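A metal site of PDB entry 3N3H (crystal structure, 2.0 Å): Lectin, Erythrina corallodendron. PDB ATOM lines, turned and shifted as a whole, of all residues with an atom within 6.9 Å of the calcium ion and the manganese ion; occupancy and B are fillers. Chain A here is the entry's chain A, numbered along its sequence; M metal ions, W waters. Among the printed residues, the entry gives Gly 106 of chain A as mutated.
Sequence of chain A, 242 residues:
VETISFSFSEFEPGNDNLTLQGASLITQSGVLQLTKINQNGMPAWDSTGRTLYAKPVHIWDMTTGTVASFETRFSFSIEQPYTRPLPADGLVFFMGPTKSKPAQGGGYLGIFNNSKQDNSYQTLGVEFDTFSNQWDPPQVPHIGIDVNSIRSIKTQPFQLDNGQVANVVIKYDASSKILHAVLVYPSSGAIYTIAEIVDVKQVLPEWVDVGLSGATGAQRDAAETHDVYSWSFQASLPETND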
ATOM      1  N   ASP A  89      -7.477  19.786  21.906  1.00  0.00           N
ATOM      2  CA  ASP A  89      -6.195  20.330  22.524  1.00  0.00           C
ATOM      3  C   ASP A  89      -6.083  19.710  23.878  1.00  0.00           C
ATOM      4  O   ASP A  89      -4.978  19.533  24.440  1.00  0.00           O
ATOM      5  CB  ASP A  89      -6.211  21.863  22.666  1.00  0.00           C
ATOM      6  CG  ASP A  89      -5.772  22.518  21.451  1.00  0.00           C
ATOM      7  OD1 ASP A  89      -4.573  22.361  21.226  1.00  0.00           O
ATOM      8  OD2 ASP A  89      -6.616  23.096  20.689  1.00  0.00           O
ATOM      9  N   GLY A  90      -7.279  19.400  24.403  1.00  0.00           N
ATOM     10  CA  GLY A  90      -7.469  18.748  25.677  1.00  0.00           C
ATOM     11  C   GLY A  90      -8.489  19.340  26.649  1.00  0.00           C
ATOM     12  O   GLY A  90      -9.324  20.198  26.324  1.00  0.00           O
ATOM     13  N   GLY A 106      -8.147  26.812  22.304  1.00  0.00           N
ATOM     14  CA  GLY A 106      -7.063  26.081  21.686  1.00  0.00           C
ATOM     15  C   GLY A 106      -6.076  25.534  22.708  1.00  0.00           C
ATOM     16  O   GLY A 106      -6.470  24.989  23.736  1.00  0.00           O
ATOM     17  N   GLY A 107      -4.789  25.676  22.407  1.00  0.00           N
ATOM     18  CA  GLY A 107      -3.746  25.177  23.300  1.00  0.00           C
ATOM     19  C   GLY A 107      -3.721  25.784  24.696  1.00  0.00           C
ATOM     20  O   GLY A 107      -3.040  25.262  25.579  1.00  0.00           O
ATOM     21  N   TYR A 108      -4.456  26.868  24.900  1.00  0.00           N
ATOM     22  CA  TYR A 108      -4.502  27.520  26.211  1.00  0.00           C
ATOM     23  C   TYR A 108      -5.587  26.928  27.083  1.00  0.00           C
ATOM     24  O   TYR A 108      -5.766  27.318  28.245  1.00  0.00           O
ATOM     25  CB  TYR A 108      -4.683  29.032  26.038  1.00  0.00           C
ATOM     26  CG  TYR A 108      -3.535  29.645  25.277  1.00  0.00           C
ATOM     27  CD1 TYR A 108      -2.229  29.583  25.773  1.00  0.00           C
ATOM     28  CD2 TYR A 108      -3.741  30.260  24.040  1.00  0.00           C
ATOM     29  CE1 TYR A 108      -1.158  30.108  25.047  1.00  0.00           C
ATOM     30  CE2 TYR A 108      -2.677  30.791  23.316  1.00  0.00           C
ATOM     31  CZ  TYR A 108      -1.385  30.706  23.821  1.00  0.00           C
ATOM     32  OH  TYR A 108      -0.335  31.219  23.097  1.00  0.00           O
ATOM     33  N   LEU A 109      -6.321  25.984  26.493  1.00  0.00           N
ATOM     34  CA  LEU A 109      -7.377  25.233  27.174  1.00  0.00           C
ATOM     35  C   LEU A 109      -8.471  26.037  27.879  1.00  0.00           C
ATOM     36  O   LEU A 109      -9.171  25.495  28.732  1.00  0.00           O
ATOM     37  CB  LEU A 109      -6.736  24.268  28.170  1.00  0.00           C
ATOM     38  CG  LEU A 109      -5.687  23.349  27.545  1.00  0.00           C
ATOM     39  CD1 LEU A 109      -5.037  22.498  28.631  1.00  0.00           C
ATOM     40  CD2 LEU A 109      -6.335  22.468  26.481  1.00  0.00           C
ATOM     41  N   GLU A 127      -3.914  19.318  33.660  1.00  0.00           N
ATOM     42  CA  GLU A 127      -4.347  19.090  32.282  1.00  0.00           C
ATOM     43  C   GLU A 127      -4.162  17.682  31.753  1.00  0.00           C
ATOM     44  O   GLU A 127      -3.394  16.862  32.302  1.00  0.00           O
ATOM     45  CB  GLU A 127      -3.618  20.062  31.352  1.00  0.00           C
ATOM     46  CG  GLU A 127      -2.105  19.818  31.394  1.00  0.00           C
ATOM     47  CD  GLU A 127      -1.308  20.565  30.343  1.00  0.00           C
ATOM     48  OE1 GLU A 127      -1.550  21.747  30.116  1.00  0.00           O
ATOM     49  OE2 GLU A 127      -0.452  19.942  29.720  1.00  0.00           O
ATOM     50  N   PHE A 128      -4.933  17.427  30.733  1.00  0.00           N
ATOM     51  CA  PHE A 128      -4.897  16.164  30.008  1.00  0.00           C
ATOM     52  C   PHE A 128      -4.827  16.730  28.594  1.00  0.00           C
ATOM     53  O   PHE A 128      -5.836  17.025  27.946  1.00  0.00           O
ATOM     54  CB  PHE A 128      -6.159  15.384  30.307  1.00  0.00           C
ATOM     55  CG  PHE A 128      -6.268  14.999  31.751  1.00  0.00           C
ATOM     56  CD1 PHE A 128      -5.625  13.861  32.223  1.00  0.00           C
ATOM     57  CD2 PHE A 128      -6.917  15.826  32.648  1.00  0.00           C
ATOM     58  CE1 PHE A 128      -5.623  13.561  33.587  1.00  0.00           C
ATOM     59  CE2 PHE A 128      -6.916  15.539  34.018  1.00  0.00           C
ATOM     60  CZ  PHE A 128      -6.264  14.400  34.479  1.00  0.00           C
ATOM     61  N   ASP A 129      -3.558  16.895  28.143  1.00  0.00           N
ATOM     62  CA  ASP A 129      -3.190  17.524  26.884  1.00  0.00           C
ATOM     63  C   ASP A 129      -3.025  16.591  25.700  1.00  0.00           C
ATOM     64  O   ASP A 129      -2.191  15.683  25.732  1.00  0.00           O
ATOM     65  CB  ASP A 129      -1.875  18.258  27.139  1.00  0.00           C
ATOM     66  CG  ASP A 129      -1.635  19.347  26.164  1.00  0.00           C
ATOM     67  OD1 ASP A 129      -2.116  19.247  25.027  1.00  0.00           O
ATOM     68  OD2 ASP A 129      -0.939  20.313  26.543  1.00  0.00           O
ATOM     69  N   THR A 130      -3.811  16.879  24.652  1.00  0.00           N
ATOM     70  CA  THR A 130      -3.735  15.981  23.469  1.00  0.00           C
ATOM     71  C   THR A 130      -2.977  16.486  22.243  1.00  0.00           C
ATOM     72  O   THR A 130      -2.792  15.747  21.286  1.00  0.00           O
ATOM     73  CB  THR A 130      -5.158  15.610  23.017  1.00  0.00           C
ATOM     74  OG1 THR A 130      -5.927  16.800  22.875  1.00  0.00           O
ATOM     75  CG2 THR A 130      -5.839  14.703  24.034  1.00  0.00           C
ATOM     76  N   PHE A 131      -2.555  17.750  22.248  1.00  0.00           N
ATOM     77  CA  PHE A 131      -1.832  18.308  21.106  1.00  0.00           C
ATOM     78  C   PHE A 131      -0.530  18.930  21.574  1.00  0.00           C
ATOM     79  O   PHE A 131      -0.515  19.659  22.542  1.00  0.00           O
ATOM     80  CB  PHE A 131      -2.666  19.400  20.418  1.00  0.00           C
ATOM     81  CG  PHE A 131      -1.992  20.020  19.227  1.00  0.00           C
ATOM     82  CD1 PHE A 131      -2.086  19.435  17.964  1.00  0.00           C
ATOM     83  CD2 PHE A 131      -1.200  21.153  19.375  1.00  0.00           C
ATOM     84  CE1 PHE A 131      -1.411  19.978  16.867  1.00  0.00           C
ATOM     85  CE2 PHE A 131      -0.514  21.704  18.295  1.00  0.00           C
ATOM     86  CZ  PHE A 131      -0.622  21.114  17.039  1.00  0.00           C
ATOM     87  N   SER A 132       0.581  18.636  20.895  1.00  0.00           N
ATOM     88  CA  SER A 132       1.868  19.175  21.303  1.00  0.00           C
ATOM     89  C   SER A 132       2.163  20.589  20.770  1.00  0.00           C
ATOM     90  O   SER A 132       2.553  20.742  19.612  1.00  0.00           O
ATOM     91  CB  SER A 132       2.981  18.227  20.863  1.00  0.00           C
ATOM     92  OG  SER A 132       4.238  18.656  21.345  1.00  0.00           O
ATOM     93  N   ASN A 133       1.966  21.611  21.609  1.00  0.00           N
ATOM     94  CA  ASN A 133       2.256  22.985  21.192  1.00  0.00           C
ATOM     95  C   ASN A 133       3.750  23.255  21.374  1.00  0.00           C
ATOM     96  O   ASN A 133       4.493  22.396  21.852  1.00  0.00           O
ATOM     97  CB  ASN A 133       1.454  24.009  22.002  1.00  0.00           C
ATOM     98  CG  ASN A 133      -0.029  23.906  21.755  1.00  0.00           C
ATOM     99  OD1 ASN A 133      -0.719  23.121  22.390  1.00  0.00           O
ATOM    100  ND2 ASN A 133      -0.539  24.706  20.826  1.00  0.00           N
ATOM    101  N   GLN A 134       4.199  24.444  20.993  1.00  0.00           N
ATOM    102  CA  GLN A 134       5.610  24.789  21.106  1.00  0.00           C
ATOM    103  C   GLN A 134       6.181  24.732  22.519  1.00  0.00           C
ATOM    104  O   GLN A 134       7.369  24.484  22.703  1.00  0.00           O
ATOM    105  CB  GLN A 134       5.870  26.157  20.486  1.00  0.00           C
ATOM    106  CG  GLN A 134       5.567  26.198  18.995  1.00  0.00           C
ATOM    107  CD  GLN A 134       6.374  25.175  18.198  1.00  0.00           C
ATOM    108  OE1 GLN A 134       5.892  24.621  17.207  1.00  0.00           O
ATOM    109  NE2 GLN A 134       7.608  24.939  18.623  1.00  0.00           N
ATOM    110  N   TRP A 135       5.328  24.942  23.520  1.00  0.00           N
ATOM    111  CA  TRP A 135       5.765  24.921  24.907  1.00  0.00           C
ATOM    112  C   TRP A 135       5.603  23.538  25.550  1.00  0.00           C
ATOM    113  O   TRP A 135       5.938  23.347  26.717  1.00  0.00           O
ATOM    114  CB  TRP A 135       4.943  25.937  25.711  1.00  0.00           C
ATOM    115  CG  TRP A 135       3.460  25.687  25.599  1.00  0.00           C
ATOM    116  CD1 TRP A 135       2.739  24.731  26.238  1.00  0.00           C
ATOM    117  CD2 TRP A 135       2.540  26.390  24.752  1.00  0.00           C
ATOM    118  NE1 TRP A 135       1.419  24.792  25.856  1.00  0.00           N
ATOM    119  CE2 TRP A 135       1.272  25.795  24.936  1.00  0.00           C
ATOM    120  CE3 TRP A 135       2.666  27.450  23.843  1.00  0.00           C
ATOM    121  CZ2 TRP A 135       0.128  26.235  24.255  1.00  0.00           C
ATOM    122  CZ3 TRP A 135       1.522  27.891  23.161  1.00  0.00           C
ATOM    123  CH2 TRP A 135       0.274  27.276  23.371  1.00  0.00           C
ATOM    124  N   ASP A 136       5.102  22.575  24.775  1.00  0.00           N
ATOM    125  CA  ASP A 136       4.866  21.212  25.261  1.00  0.00           C
ATOM    126  C   ASP A 136       5.975  20.223  24.982  1.00  0.00           C
ATOM    127  O   ASP A 136       6.822  20.441  24.120  1.00  0.00           O
ATOM    128  CB  ASP A 136       3.632  20.591  24.603  1.00  0.00           C
ATOM    129  CG  ASP A 136       2.347  21.091  25.188  1.00  0.00           C
ATOM    130  OD1 ASP A 136       2.299  21.338  26.408  1.00  0.00           O
ATOM    131  OD2 ASP A 136       1.379  21.213  24.422  1.00  0.00           O
ATOM    132  N   PRO A 137       5.979  19.130  25.735  1.00  0.00           N
ATOM    133  CA  PRO A 137       6.998  18.101  25.506  1.00  0.00           C
ATOM    134  C   PRO A 137       6.467  17.459  24.230  1.00  0.00           C
ATOM    135  O   PRO A 137       5.284  17.626  23.886  1.00  0.00           O
ATOM    136  CB  PRO A 137       6.849  17.189  26.728  1.00  0.00           C
ATOM    137  CG  PRO A 137       5.404  17.369  27.129  1.00  0.00           C
ATOM    138  CD  PRO A 137       5.224  18.859  26.967  1.00  0.00           C
ATOM    139  N   VAL A 140       2.379  13.215  23.410  1.00  0.00           N
ATOM    140  CA  VAL A 140       0.981  13.487  23.671  1.00  0.00           C
ATOM    141  C   VAL A 140       0.228  12.173  23.493  1.00  0.00           C
ATOM    142  O   VAL A 140       0.608  11.340  22.685  1.00  0.00           O
ATOM    143  CB  VAL A 140       0.377  14.558  22.714  1.00  0.00           C
ATOM    144  CG1 VAL A 140       0.854  15.938  23.113  1.00  0.00           C
ATOM    145  CG2 VAL A 140       0.757  14.255  21.273  1.00  0.00           C
ATOM    146  N   HIS A 142      -0.518  13.848  27.421  1.00  0.00           N
ATOM    147  CA  HIS A 142       0.235  13.853  28.667  1.00  0.00           C
ATOM    148  C   HIS A 142      -0.546  14.566  29.763  1.00  0.00           C
ATOM    149  O   HIS A 142      -1.407  15.399  29.491  1.00  0.00           O
ATOM    150  CB  HIS A 142       1.596  14.524  28.488  1.00  0.00           C
ATOM    151  CG  HIS A 142       1.536  15.944  27.985  1.00  0.00           C
ATOM    152  ND1 HIS A 142       1.734  16.271  26.666  1.00  0.00           N
ATOM    153  CD2 HIS A 142       1.275  17.104  28.631  1.00  0.00           C
ATOM    154  CE1 HIS A 142       1.602  17.579  26.508  1.00  0.00           C
ATOM    155  NE2 HIS A 142       1.324  18.104  27.693  1.00  0.00           N
ATOM    156  N   ILE A 143      -0.257  14.193  30.996  1.00  0.00           N
ATOM    157  CA  ILE A 143      -0.888  14.828  32.142  1.00  0.00           C
ATOM    158  C   ILE A 143       0.116  15.915  32.501  1.00  0.00           C
ATOM    159  O   ILE A 143       1.318  15.711  32.388  1.00  0.00           O
ATOM    160  CB  ILE A 143      -1.004  13.882  33.347  1.00  0.00           C
ATOM    161  CG1 ILE A 143      -1.752  12.607  32.938  1.00  0.00           C
ATOM    162  CG2 ILE A 143      -1.719  14.598  34.486  1.00  0.00           C
ATOM    163  CD1 ILE A 143      -1.691  11.506  33.969  1.00  0.00           C
ATOM    164  N   GLY A 144      -0.381  17.072  32.930  1.00  0.00           N
ATOM    165  CA  GLY A 144       0.530  18.132  33.300  1.00  0.00           C
ATOM    166  C   GLY A 144       0.026  18.906  34.490  1.00  0.00           C
ATOM    167  O   GLY A 144      -1.180  19.036  34.676  1.00  0.00           O
ATOM    168  N   ASP A 146      -0.071  22.489  35.926  1.00  0.00           N
ATOM    169  CA  ASP A 146       0.142  23.868  35.494  1.00  0.00           C
ATOM    170  C   ASP A 146       0.001  24.851  36.638  1.00  0.00           C
ATOM    171  O   ASP A 146      -1.040  24.914  37.297  1.00  0.00           O
ATOM    172  CB  ASP A 146      -0.842  24.243  34.385  1.00  0.00           C
ATOM    173  CG  ASP A 146      -0.775  23.302  33.189  1.00  0.00           C
ATOM    174  OD1 ASP A 146       0.240  22.589  33.035  1.00  0.00           O
ATOM    175  OD2 ASP A 146      -1.735  23.292  32.383  1.00  0.00           O
ATOM    176  N   ILE A 150       0.806  27.798  31.094  1.00  0.00           N
ATOM    177  CA  ILE A 150       0.386  26.656  30.294  1.00  0.00           C
ATOM    178  C   ILE A 150       1.582  25.715  30.142  1.00  0.00           C
ATOM    179  O   ILE A 150       1.434  24.545  29.788  1.00  0.00           O
ATOM    180  CB  ILE A 150      -0.118  27.121  28.898  1.00  0.00           C
ATOM    181  CG1 ILE A 150      -0.751  25.939  28.160  1.00  0.00           C
ATOM    182  CG2 ILE A 150       1.036  27.724  28.097  1.00  0.00           C
ATOM    183  CD1 ILE A 150      -2.034  25.417  28.811  1.00  0.00           C
ATOM    184  N   ARG A 151       2.771  26.241  30.431  1.00  0.00           N
ATOM    185  CA  ARG A 151       3.995  25.440  30.373  1.00  0.00           C
ATOM    186  C   ARG A 151       4.091  24.739  31.736  1.00  0.00           C
ATOM    187  O   ARG A 151       4.475  25.347  32.738  1.00  0.00           O
ATOM    188  CB  ARG A 151       5.212  26.346  30.129  1.00  0.00           C
ATOM    189  CG  ARG A 151       6.536  25.589  30.048  1.00  0.00           C
ATOM    190  CD  ARG A 151       7.740  26.503  29.785  1.00  0.00           C
ATOM    191  NE  ARG A 151       7.940  26.791  28.363  1.00  0.00           N
ATOM    192  CZ  ARG A 151       7.393  27.810  27.705  1.00  0.00           C
ATOM    193  NH1 ARG A 151       6.599  28.658  28.335  1.00  0.00           N
ATOM    194  NH2 ARG A 151       7.657  27.970  26.413  1.00  0.00           N
ATOM    195  N   SER A 152       3.745  23.464  31.755  1.00  0.00           N
ATOM    196  CA  SER A 152       3.732  22.653  32.977  1.00  0.00           C
ATOM    197  C   SER A 152       5.057  22.562  33.723  1.00  0.00           C
ATOM    198  O   SER A 152       6.132  22.524  33.116  1.00  0.00           O
ATOM    199  CB  SER A 152       3.270  21.229  32.647  1.00  0.00           C
ATOM    200  OG  SER A 152       2.090  21.255  31.866  1.00  0.00           O
ATOM    201  N   THR A 155       5.232  16.951  33.703  1.00  0.00           N
ATOM    202  CA  THR A 155       4.327  16.214  32.825  1.00  0.00           C
ATOM    203  C   THR A 155       4.562  14.713  32.905  1.00  0.00           C
ATOM    204  O   THR A 155       5.627  14.257  33.328  1.00  0.00           O
ATOM    205  CB  THR A 155       4.495  16.640  31.351  1.00  0.00           C
ATOM    206  OG1 THR A 155       5.841  16.388  30.924  1.00  0.00           O
ATOM    207  CG2 THR A 155       4.181  18.127  31.175  1.00  0.00           C
HETATM  208 CA    CA M   1      -1.030  21.398  24.210  1.00  0.00          CA
HETATM  209 MN    MN M   2       0.786  20.378  27.920  1.00  0.00          MN
HETATM  210  O   HOH W   1       2.703  20.734  29.364  1.00  0.00           O
HETATM  211  O   HOH W   2      -1.331  23.232  25.939  1.00  0.00           O
HETATM  212  O   HOH W   3      -3.433  21.467  23.518  1.00  0.00           O
HETATM  213  O   HOH W   4       0.081  22.721  28.345  1.00  0.00           O
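Water W2 lies within hydrogen-bond range of O of Gly 107 (2.7 Å) and NE1 of Trp 135 (3.2 Å). Water W4 lies within hydrogen-bond range of OE1 of Glu 127 (2.6 Å) and O of Ile 150 (2.7 Å).
OD2 of Asp 136 is bound to the calcium ion. The backbone carbonyl oxygen (O) of Phe 131 is bound to the calcium ion, at 2.5 Å. The calcium ion is bound by water W3 (2.5 Å). OD1 of Asn 133 binds the calcium ion. The calcium ion is bound by water W2, 2.5 Å away. OD1 of Asp 129 is bound to the calcium ion. The side-chain carboxylate (OD2) of Asp 129 is bound to the calcium ion, 2.6 Å away.
The side-chain carboxylate (OE1) of Glu 127 sits close to the side-chain carboxylate (OD2) of Asp 146, at 2.7 Å. O of Gly 144 is in hydrogen-bond range of N of Glu 127, 2.9 Å away.
Four residues have an atom within 4 Å of the manganese ion: Glu 127, Asp 129, Asp 136 and His 142. The nearest printed residue that does not touch the manganese ion is Ser 152 (4.2 Å).
The manganese ion is bound by the side-chain carboxylate of Asp 129 (2.2 Å), the side-chain carboxylate of Glu 127 (2.2 Å), the side-chain carboxylate of Asp 136 (2.3 Å), a ring nitrogen (NE2) of His 142 (2.3 Å), water W1 (2.4 Å) and water W4 (2.5 Å).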
